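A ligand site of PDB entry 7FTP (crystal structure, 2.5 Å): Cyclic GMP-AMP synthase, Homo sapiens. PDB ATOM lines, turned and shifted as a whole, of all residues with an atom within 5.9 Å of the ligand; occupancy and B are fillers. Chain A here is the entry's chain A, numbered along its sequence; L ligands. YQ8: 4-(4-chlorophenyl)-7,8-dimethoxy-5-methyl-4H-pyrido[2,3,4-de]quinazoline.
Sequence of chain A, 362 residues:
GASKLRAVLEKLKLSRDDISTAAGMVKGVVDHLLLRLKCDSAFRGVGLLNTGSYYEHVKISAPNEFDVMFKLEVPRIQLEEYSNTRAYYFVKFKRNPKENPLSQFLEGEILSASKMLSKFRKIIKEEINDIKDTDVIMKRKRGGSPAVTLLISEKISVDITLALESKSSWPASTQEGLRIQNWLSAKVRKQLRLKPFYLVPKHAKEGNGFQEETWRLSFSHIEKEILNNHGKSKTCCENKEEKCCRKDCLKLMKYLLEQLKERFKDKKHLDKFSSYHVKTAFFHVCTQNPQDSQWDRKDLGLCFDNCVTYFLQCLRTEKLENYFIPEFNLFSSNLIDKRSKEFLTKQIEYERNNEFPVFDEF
N14 of the ligand is in hydrogen-bond range of NH2 of Arg 216 (3.2 Å). An oxygen (O21) of the ligand sits close to the side-chain hydroxyl (OH) of Tyr 276 (3.5 Å). The side-chain amide nitrogen (ND2) of Asn 322 sits at hydrogen-bond distance from an oxygen (O20) of the ligand, at 2.8 Å.
OD1 of Asn 322 is in hydrogen-bond range of N of Ile 325 (2.8 Å). N of Asn 322 is in hydrogen-bond range of O of Phe 328, 2.8 Å away. The backbone NH (N) of Tyr 276 lies close to the side-chain hydroxyl (OG) of Ser 274, 3.2 Å away. ND2 of Asn 322 is in hydrogen-bond range of OH of Tyr 276 (3.5 Å). A ring nitrogen (ND1) of His 277 sits at hydrogen-bond distance from the backbone NH (N) of Ser 274, at 2.9 Å. OD1 of Asn 322 lies within hydrogen-bond range of N of Phe 324 (2.9 Å). The backbone carbonyl oxygen of Ala 87 lies within hydrogen-bond range of the backbone NH of Leu 217, 3.3 Å away.
Merely in contact with the ligand: Lys 272 (3.2 Å), Ala 87 (3.3 Å), Leu 217 (3.3 Å), His 277 (3.4 Å), Leu 330 (3.4 Å), Asp 271 (3.4 Å), Ser 274 (3.4 Å), Ile 325 (3.7 Å), Phe 328 (3.8 Å) and Phe 219 (3.96 Å). Hydrophobic or aromatic side chains within 4 Å of the ligand: Ala 87, Phe 219, Tyr 276, His 277, Ile 325, Phe 328 and Leu 330. Of the 21 residues printed, 13 come within 4 Å of the ligand. The nearest printed residue that does not touch the ligand is Phe 273 (4.2 Å).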
ATOM      1  N   ALA A  87     -16.499  29.418  32.029  1.00  0.00           N
ATOM      2  CA  ALA A  87     -17.189  28.415  31.214  1.00  0.00           C
ATOM      3  C   ALA A  87     -17.707  27.148  31.949  1.00  0.00           C
ATOM      4  O   ALA A  87     -18.612  26.479  31.428  1.00  0.00           O
ATOM      5  CB  ALA A  87     -16.293  27.996  30.087  1.00  0.00           C
ATOM      6  N   TYR A  88     -17.089  26.797  33.107  1.00  0.00           N
ATOM      7  CA  TYR A  88     -17.394  25.589  33.855  1.00  0.00           C
ATOM      8  C   TYR A  88     -18.176  25.947  35.092  1.00  0.00           C
ATOM      9  O   TYR A  88     -17.794  26.843  35.849  1.00  0.00           O
ATOM     10  CB  TYR A  88     -16.119  24.772  34.149  1.00  0.00           C
ATOM     11  CG  TYR A  88     -15.411  24.288  32.897  1.00  0.00           C
ATOM     12  CD1 TYR A  88     -14.452  25.071  32.268  1.00  0.00           C
ATOM     13  CD2 TYR A  88     -15.697  23.042  32.347  1.00  0.00           C
ATOM     14  CE1 TYR A  88     -13.815  24.653  31.096  1.00  0.00           C
ATOM     15  CE2 TYR A  88     -15.039  22.587  31.193  1.00  0.00           C
ATOM     16  CZ  TYR A  88     -14.103  23.397  30.567  1.00  0.00           C
ATOM     17  OH  TYR A  88     -13.471  22.978  29.419  1.00  0.00           O
ATOM     18  N   LYS A 202     -18.203  17.854  31.206  1.00  0.00           N
ATOM     19  CA  LYS A 202     -16.794  17.989  30.846  1.00  0.00           C
ATOM     20  C   LYS A 202     -16.131  18.541  32.093  1.00  0.00           C
ATOM     21  O   LYS A 202     -16.356  19.695  32.475  1.00  0.00           O
ATOM     22  CB  LYS A 202     -16.613  18.931  29.635  1.00  0.00           C
ATOM     23  CG  LYS A 202     -17.139  18.367  28.324  1.00  0.00           C
ATOM     24  CD  LYS A 202     -16.148  17.421  27.634  1.00  0.00           C
ATOM     25  CE  LYS A 202     -16.650  17.004  26.273  1.00  0.00           C
ATOM     26  NZ  LYS A 202     -15.651  17.314  25.196  1.00  0.00           N
ATOM     27  N   ARG A 216     -19.712  22.227  31.320  1.00  0.00           N
ATOM     28  CA  ARG A 216     -19.288  23.306  30.411  1.00  0.00           C
ATOM     29  C   ARG A 216     -20.450  23.725  29.517  1.00  0.00           C
ATOM     30  O   ARG A 216     -21.197  22.855  29.040  1.00  0.00           O
ATOM     31  CB  ARG A 216     -18.138  22.803  29.525  1.00  0.00           C
ATOM     32  CG  ARG A 216     -17.444  23.837  28.639  1.00  0.00           C
ATOM     33  CD  ARG A 216     -16.776  23.135  27.474  1.00  0.00           C
ATOM     34  NE  ARG A 216     -17.745  22.794  26.424  1.00  0.00           N
ATOM     35  CZ  ARG A 216     -17.665  21.721  25.637  1.00  0.00           C
ATOM     36  NH1 ARG A 216     -16.662  20.858  25.772  1.00  0.00           N
ATOM     37  NH2 ARG A 216     -18.593  21.504  24.705  1.00  0.00           N
ATOM     38  N   LEU A 217     -20.573  25.040  29.262  1.00  0.00           N
ATOM     39  CA  LEU A 217     -21.602  25.611  28.387  1.00  0.00           C
ATOM     40  C   LEU A 217     -21.483  25.085  26.945  1.00  0.00           C
ATOM     41  O   LEU A 217     -20.374  24.845  26.444  1.00  0.00           O
ATOM     42  CB  LEU A 217     -21.531  27.147  28.358  1.00  0.00           C
ATOM     43  CG  LEU A 217     -21.616  27.903  29.687  1.00  0.00           C
ATOM     44  CD1 LEU A 217     -21.511  29.403  29.457  1.00  0.00           C
ATOM     45  CD2 LEU A 217     -22.910  27.609  30.432  1.00  0.00           C
ATOM     46  N   SER A 218     -22.653  24.861  26.304  1.00  0.00           N
ATOM     47  CA  SER A 218     -22.752  24.405  24.909  1.00  0.00           C
ATOM     48  C   SER A 218     -23.687  25.346  24.123  1.00  0.00           C
ATOM     49  O   SER A 218     -24.735  25.730  24.643  1.00  0.00           O
ATOM     50  CB  SER A 218     -23.203  22.951  24.833  1.00  0.00           C
ATOM     51  OG  SER A 218     -22.579  22.275  23.754  1.00  0.00           O
ATOM     52  N   PHE A 219     -23.250  25.768  22.929  1.00  0.00           N
ATOM     53  CA  PHE A 219     -23.980  26.648  22.008  1.00  0.00           C
ATOM     54  C   PHE A 219     -23.946  26.092  20.582  1.00  0.00           C
ATOM     55  O   PHE A 219     -24.160  26.831  19.609  1.00  0.00           O
ATOM     56  CB  PHE A 219     -23.418  28.074  22.059  1.00  0.00           C
ATOM     57  CG  PHE A 219     -23.507  28.752  23.402  1.00  0.00           C
ATOM     58  CD1 PHE A 219     -24.710  29.314  23.835  1.00  0.00           C
ATOM     59  CD2 PHE A 219     -22.388  28.852  24.232  1.00  0.00           C
ATOM     60  CE1 PHE A 219     -24.797  29.932  25.094  1.00  0.00           C
ATOM     61  CE2 PHE A 219     -22.472  29.503  25.474  1.00  0.00           C
ATOM     62  CZ  PHE A 219     -23.677  30.020  25.903  1.00  0.00           C
ATOM     63  N   GLU A 223     -24.509  27.987  16.835  1.00  0.00           N
ATOM     64  CA  GLU A 223     -23.469  27.859  15.820  1.00  0.00           C
ATOM     65  C   GLU A 223     -24.006  27.293  14.528  1.00  0.00           C
ATOM     66  O   GLU A 223     -23.692  27.838  13.460  1.00  0.00           O
ATOM     67  CB  GLU A 223     -22.326  26.993  16.341  1.00  0.00           C
ATOM     68  CG  GLU A 223     -21.499  27.658  17.430  1.00  0.00           C
ATOM     69  CD  GLU A 223     -20.629  26.720  18.242  1.00  0.00           C
ATOM     70  OE1 GLU A 223     -20.512  25.530  17.855  1.00  0.00           O
ATOM     71  OE2 GLU A 223     -20.060  27.165  19.272  1.00  0.00           O
ATOM     72  N   LYS A 261      -3.730  16.615  11.719  1.00  0.00           N
ATOM     73  CA  LYS A 261      -3.906  15.772  12.919  1.00  0.00           C
ATOM     74  C   LYS A 261      -3.672  14.284  12.606  1.00  0.00           C
ATOM     75  O   LYS A 261      -3.075  13.574  13.423  1.00  0.00           O
ATOM     76  CB  LYS A 261      -5.295  15.957  13.562  1.00  0.00           C
ATOM     77  CG  LYS A 261      -5.497  17.284  14.312  1.00  0.00           C
ATOM     78  CD  LYS A 261      -6.751  17.259  15.249  1.00  0.00           C
ATOM     79  CE  LYS A 261      -6.422  16.490  16.513  1.00  0.00           C
ATOM     80  NZ  LYS A 261      -7.529  16.444  17.498  1.00  0.00           N
ATOM     81  N   ASP A 271      -2.949  16.958  19.608  1.00  0.00           N
ATOM     82  CA  ASP A 271      -3.957  16.314  20.456  1.00  0.00           C
ATOM     83  C   ASP A 271      -4.895  17.316  21.109  1.00  0.00           C
ATOM     84  O   ASP A 271      -6.049  16.976  21.367  1.00  0.00           O
ATOM     85  CB  ASP A 271      -3.257  15.495  21.557  1.00  0.00           C
ATOM     86  CG  ASP A 271      -2.756  14.108  21.182  1.00  0.00           C
ATOM     87  OD1 ASP A 271      -2.920  13.719  20.002  1.00  0.00           O
ATOM     88  OD2 ASP A 271      -2.201  13.411  22.064  1.00  0.00           O
ATOM     89  N   LYS A 272      -4.404  18.526  21.384  1.00  0.00           N
ATOM     90  CA  LYS A 272      -5.200  19.551  22.043  1.00  0.00           C
ATOM     91  C   LYS A 272      -5.990  20.366  21.059  1.00  0.00           C
ATOM     92  O   LYS A 272      -6.893  21.083  21.479  1.00  0.00           O
ATOM     93  CB  LYS A 272      -4.332  20.462  22.923  1.00  0.00           C
ATOM     94  CG  LYS A 272      -3.568  19.726  24.029  1.00  0.00           C
ATOM     95  CD  LYS A 272      -4.355  19.549  25.312  1.00  0.00           C
ATOM     96  CE  LYS A 272      -3.662  18.612  26.280  1.00  0.00           C
ATOM     97  NZ  LYS A 272      -2.526  19.271  26.978  1.00  0.00           N
ATOM     98  N   PHE A 273      -5.679  20.272  19.750  1.00  0.00           N
ATOM     99  CA  PHE A 273      -6.401  21.022  18.727  1.00  0.00           C
ATOM    100  C   PHE A 273      -7.595  20.273  18.195  1.00  0.00           C
ATOM    101  O   PHE A 273      -7.528  19.087  17.974  1.00  0.00           O
ATOM    102  CB  PHE A 273      -5.478  21.430  17.579  1.00  0.00           C
ATOM    103  CG  PHE A 273      -4.371  22.367  17.995  1.00  0.00           C
ATOM    104  CD1 PHE A 273      -4.621  23.734  18.154  1.00  0.00           C
ATOM    105  CD2 PHE A 273      -3.079  21.889  18.200  1.00  0.00           C
ATOM    106  CE1 PHE A 273      -3.596  24.606  18.522  1.00  0.00           C
ATOM    107  CE2 PHE A 273      -2.050  22.758  18.598  1.00  0.00           C
ATOM    108  CZ  PHE A 273      -2.315  24.118  18.741  1.00  0.00           C
ATOM    109  N   SER A 274      -8.682  20.987  17.950  1.00  0.00           N
ATOM    110  CA  SER A 274      -9.895  20.365  17.409  1.00  0.00           C
ATOM    111  C   SER A 274     -10.610  21.314  16.475  1.00  0.00           C
ATOM    112  O   SER A 274     -10.297  22.503  16.434  1.00  0.00           O
ATOM    113  CB  SER A 274     -10.800  19.846  18.534  1.00  0.00           C
ATOM    114  OG  SER A 274     -11.803  20.762  18.965  1.00  0.00           O
ATOM    115  N   TYR A 276     -13.231  22.694  16.810  1.00  0.00           N
ATOM    116  CA  TYR A 276     -13.865  23.760  17.558  1.00  0.00           C
ATOM    117  C   TYR A 276     -12.986  25.057  17.479  1.00  0.00           C
ATOM    118  O   TYR A 276     -13.506  26.185  17.342  1.00  0.00           O
ATOM    119  CB  TYR A 276     -14.138  23.359  19.016  1.00  0.00           C
ATOM    120  CG  TYR A 276     -14.951  24.430  19.709  1.00  0.00           C
ATOM    121  CD1 TYR A 276     -16.277  24.669  19.324  1.00  0.00           C
ATOM    122  CD2 TYR A 276     -14.387  25.264  20.654  1.00  0.00           C
ATOM    123  CE1 TYR A 276     -17.027  25.675  19.931  1.00  0.00           C
ATOM    124  CE2 TYR A 276     -15.121  26.287  21.257  1.00  0.00           C
ATOM    125  CZ  TYR A 276     -16.444  26.479  20.898  1.00  0.00           C
ATOM    126  OH  TYR A 276     -17.196  27.478  21.471  1.00  0.00           O
ATOM    127  N   HIS A 277     -11.654  24.874  17.537  1.00  0.00           N
ATOM    128  CA  HIS A 277     -10.690  25.951  17.391  1.00  0.00           C
ATOM    129  C   HIS A 277     -10.816  26.648  16.010  1.00  0.00           C
ATOM    130  O   HIS A 277     -10.884  27.874  15.931  1.00  0.00           O
ATOM    131  CB  HIS A 277      -9.264  25.420  17.586  1.00  0.00           C
ATOM    132  CG  HIS A 277      -9.015  24.869  18.947  1.00  0.00           C
ATOM    133  ND1 HIS A 277      -8.372  23.672  19.124  1.00  0.00           N
ATOM    134  CD2 HIS A 277      -9.307  25.390  20.158  1.00  0.00           C
ATOM    135  CE1 HIS A 277      -8.280  23.503  20.427  1.00  0.00           C
ATOM    136  NE2 HIS A 277      -8.851  24.503  21.090  1.00  0.00           N
ATOM    137  N   ASN A 322     -12.971  32.501  23.051  1.00  0.00           N
ATOM    138  CA  ASN A 322     -14.209  31.759  22.820  1.00  0.00           C
ATOM    139  C   ASN A 322     -15.213  32.803  22.313  1.00  0.00           C
ATOM    140  O   ASN A 322     -15.318  33.920  22.871  1.00  0.00           O
ATOM    141  CB  ASN A 322     -14.693  31.104  24.127  1.00  0.00           C
ATOM    142  CG  ASN A 322     -15.955  30.315  24.017  1.00  0.00           C
ATOM    143  OD1 ASN A 322     -17.041  30.839  23.781  1.00  0.00           O
ATOM    144  ND2 ASN A 322     -15.854  29.037  24.255  1.00  0.00           N
ATOM    145  N   PHE A 324     -18.416  32.954  22.365  1.00  0.00           N
ATOM    146  CA  PHE A 324     -19.553  33.129  23.242  1.00  0.00           C
ATOM    147  C   PHE A 324     -19.128  33.670  24.592  1.00  0.00           C
ATOM    148  O   PHE A 324     -19.851  34.492  25.188  1.00  0.00           O
ATOM    149  CB  PHE A 324     -20.286  31.802  23.406  1.00  0.00           C
ATOM    150  CG  PHE A 324     -21.006  31.378  22.152  1.00  0.00           C
ATOM    151  CD1 PHE A 324     -20.389  30.559  21.209  1.00  0.00           C
ATOM    152  CD2 PHE A 324     -22.312  31.792  21.907  1.00  0.00           C
ATOM    153  CE1 PHE A 324     -21.041  30.207  20.027  1.00  0.00           C
ATOM    154  CE2 PHE A 324     -22.965  31.441  20.724  1.00  0.00           C
ATOM    155  CZ  PHE A 324     -22.322  30.642  19.800  1.00  0.00           C
ATOM    156  N   ILE A 325     -17.932  33.211  25.069  1.00  0.00           N
ATOM    157  CA  ILE A 325     -17.305  33.567  26.363  1.00  0.00           C
ATOM    158  C   ILE A 325     -15.962  34.325  26.041  1.00  0.00           C
ATOM    159  O   ILE A 325     -14.890  33.701  25.995  1.00  0.00           O
ATOM    160  CB  ILE A 325     -17.135  32.267  27.236  1.00  0.00           C
ATOM    161  CG1 ILE A 325     -18.434  31.423  27.301  1.00  0.00           C
ATOM    162  CG2 ILE A 325     -16.698  32.624  28.634  1.00  0.00           C
ATOM    163  CD1 ILE A 325     -18.316  29.992  26.843  1.00  0.00           C
ATOM    164  N   PHE A 328     -12.698  33.792  27.889  1.00  0.00           N
ATOM    165  CA  PHE A 328     -12.165  32.445  27.851  1.00  0.00           C
ATOM    166  C   PHE A 328     -11.268  32.370  26.641  1.00  0.00           C
ATOM    167  O   PHE A 328     -11.723  32.524  25.519  1.00  0.00           O
ATOM    168  CB  PHE A 328     -13.278  31.372  27.805  1.00  0.00           C
ATOM    169  CG  PHE A 328     -12.748  29.974  28.000  1.00  0.00           C
ATOM    170  CD1 PHE A 328     -12.799  29.362  29.241  1.00  0.00           C
ATOM    171  CD2 PHE A 328     -12.166  29.274  26.944  1.00  0.00           C
ATOM    172  CE1 PHE A 328     -12.275  28.073  29.423  1.00  0.00           C
ATOM    173  CE2 PHE A 328     -11.640  27.999  27.124  1.00  0.00           C
ATOM    174  CZ  PHE A 328     -11.695  27.404  28.374  1.00  0.00           C
ATOM    175  N   LEU A 330      -9.042  30.031  24.440  1.00  0.00           N
ATOM    176  CA  LEU A 330      -8.784  28.664  24.017  1.00  0.00           C
ATOM    177  C   LEU A 330      -7.274  28.389  23.740  1.00  0.00           C
ATOM    178  O   LEU A 330      -6.868  27.231  23.701  1.00  0.00           O
ATOM    179  CB  LEU A 330      -9.637  28.356  22.762  1.00  0.00           C
ATOM    180  CG  LEU A 330     -11.172  28.451  22.906  1.00  0.00           C
ATOM    181  CD1 LEU A 330     -11.836  28.873  21.609  1.00  0.00           C
ATOM    182  CD2 LEU A 330     -11.755  27.136  23.389  1.00  0.00           C
ATOM    183  N   LEU A 335      -4.067  25.859  28.553  1.00  0.00           N
ATOM    184  CA  LEU A 335      -4.861  24.933  27.760  1.00  0.00           C
ATOM    185  C   LEU A 335      -3.994  24.217  26.744  1.00  0.00           C
ATOM    186  O   LEU A 335      -3.984  22.986  26.692  1.00  0.00           O
ATOM    187  CB  LEU A 335      -6.019  25.667  27.063  1.00  0.00           C
ATOM    188  CG  LEU A 335      -7.284  25.831  27.897  1.00  0.00           C
ATOM    189  CD1 LEU A 335      -8.303  26.598  27.140  1.00  0.00           C
ATOM    190  CD2 LEU A 335      -7.873  24.460  28.307  1.00  0.00           C
HETATM  191  C10 YQ8 L   1     -11.024  19.495  23.501  1.00  0.00           C
HETATM  192  C11 YQ8 L   1     -10.157  21.152  21.970  1.00  0.00           C
HETATM  193  C13 YQ8 L   1     -16.348  23.770  23.286  1.00  0.00           C
HETATM  194  C15 YQ8 L   1     -15.924  21.839  22.141  1.00  0.00           C
HETATM  195  C17 YQ8 L   1     -15.510  25.790  25.044  1.00  0.00           C
HETATM  196  C18 YQ8 L   1     -16.805  25.820  24.476  1.00  0.00           C
HETATM  197  C19 YQ8 L   1     -17.237  24.808  23.672  1.00  0.00           C
HETATM  198  C22 YQ8 L   1     -18.896  27.000  24.371  1.00  0.00           C
HETATM  199  C24 YQ8 L   1     -15.286  26.803  27.209  1.00  0.00           C
HETATM  200  C25 YQ8 L   1     -11.027  23.612  25.389  1.00  0.00           C
HETATM  201  C1  YQ8 L   1     -14.601  24.801  24.707  1.00  0.00           C
HETATM  202  C2  YQ8 L   1     -15.049  23.746  23.846  1.00  0.00           C
HETATM  203  C3  YQ8 L   1     -14.225  22.750  23.456  1.00  0.00           C
HETATM  204  N4  YQ8 L   1     -12.905  22.689  23.963  1.00  0.00           N
HETATM  205  C5  YQ8 L   1     -12.428  23.709  24.863  1.00  0.00           C
HETATM  206  C6  YQ8 L   1     -13.260  24.702  25.231  1.00  0.00           C
HETATM  207  C7  YQ8 L   1     -11.990  21.708  23.436  1.00  0.00           C
HETATM  208  C8  YQ8 L   1     -11.108  22.052  22.413  1.00  0.00           C
HETATM  209  C9  YQ8 L   1     -10.119  19.880  22.522  1.00  0.00           C
HETATM  210  C12 YQ8 L   1     -11.940  20.418  23.985  1.00  0.00           C
HETATM  211  N14 YQ8 L   1     -16.804  22.791  22.430  1.00  0.00           N
HETATM  212  N16 YQ8 L   1     -14.673  21.672  22.593  1.00  0.00           N
HETATM  213  O20 YQ8 L   1     -15.065  26.864  25.802  1.00  0.00           O
HETATM  214  O21 YQ8 L   1     -17.559  26.903  24.865  1.00  0.00           O
HETATM  215 CL23 YQ8 L   1      -8.955  18.723  21.924  1.00  0.00          CL
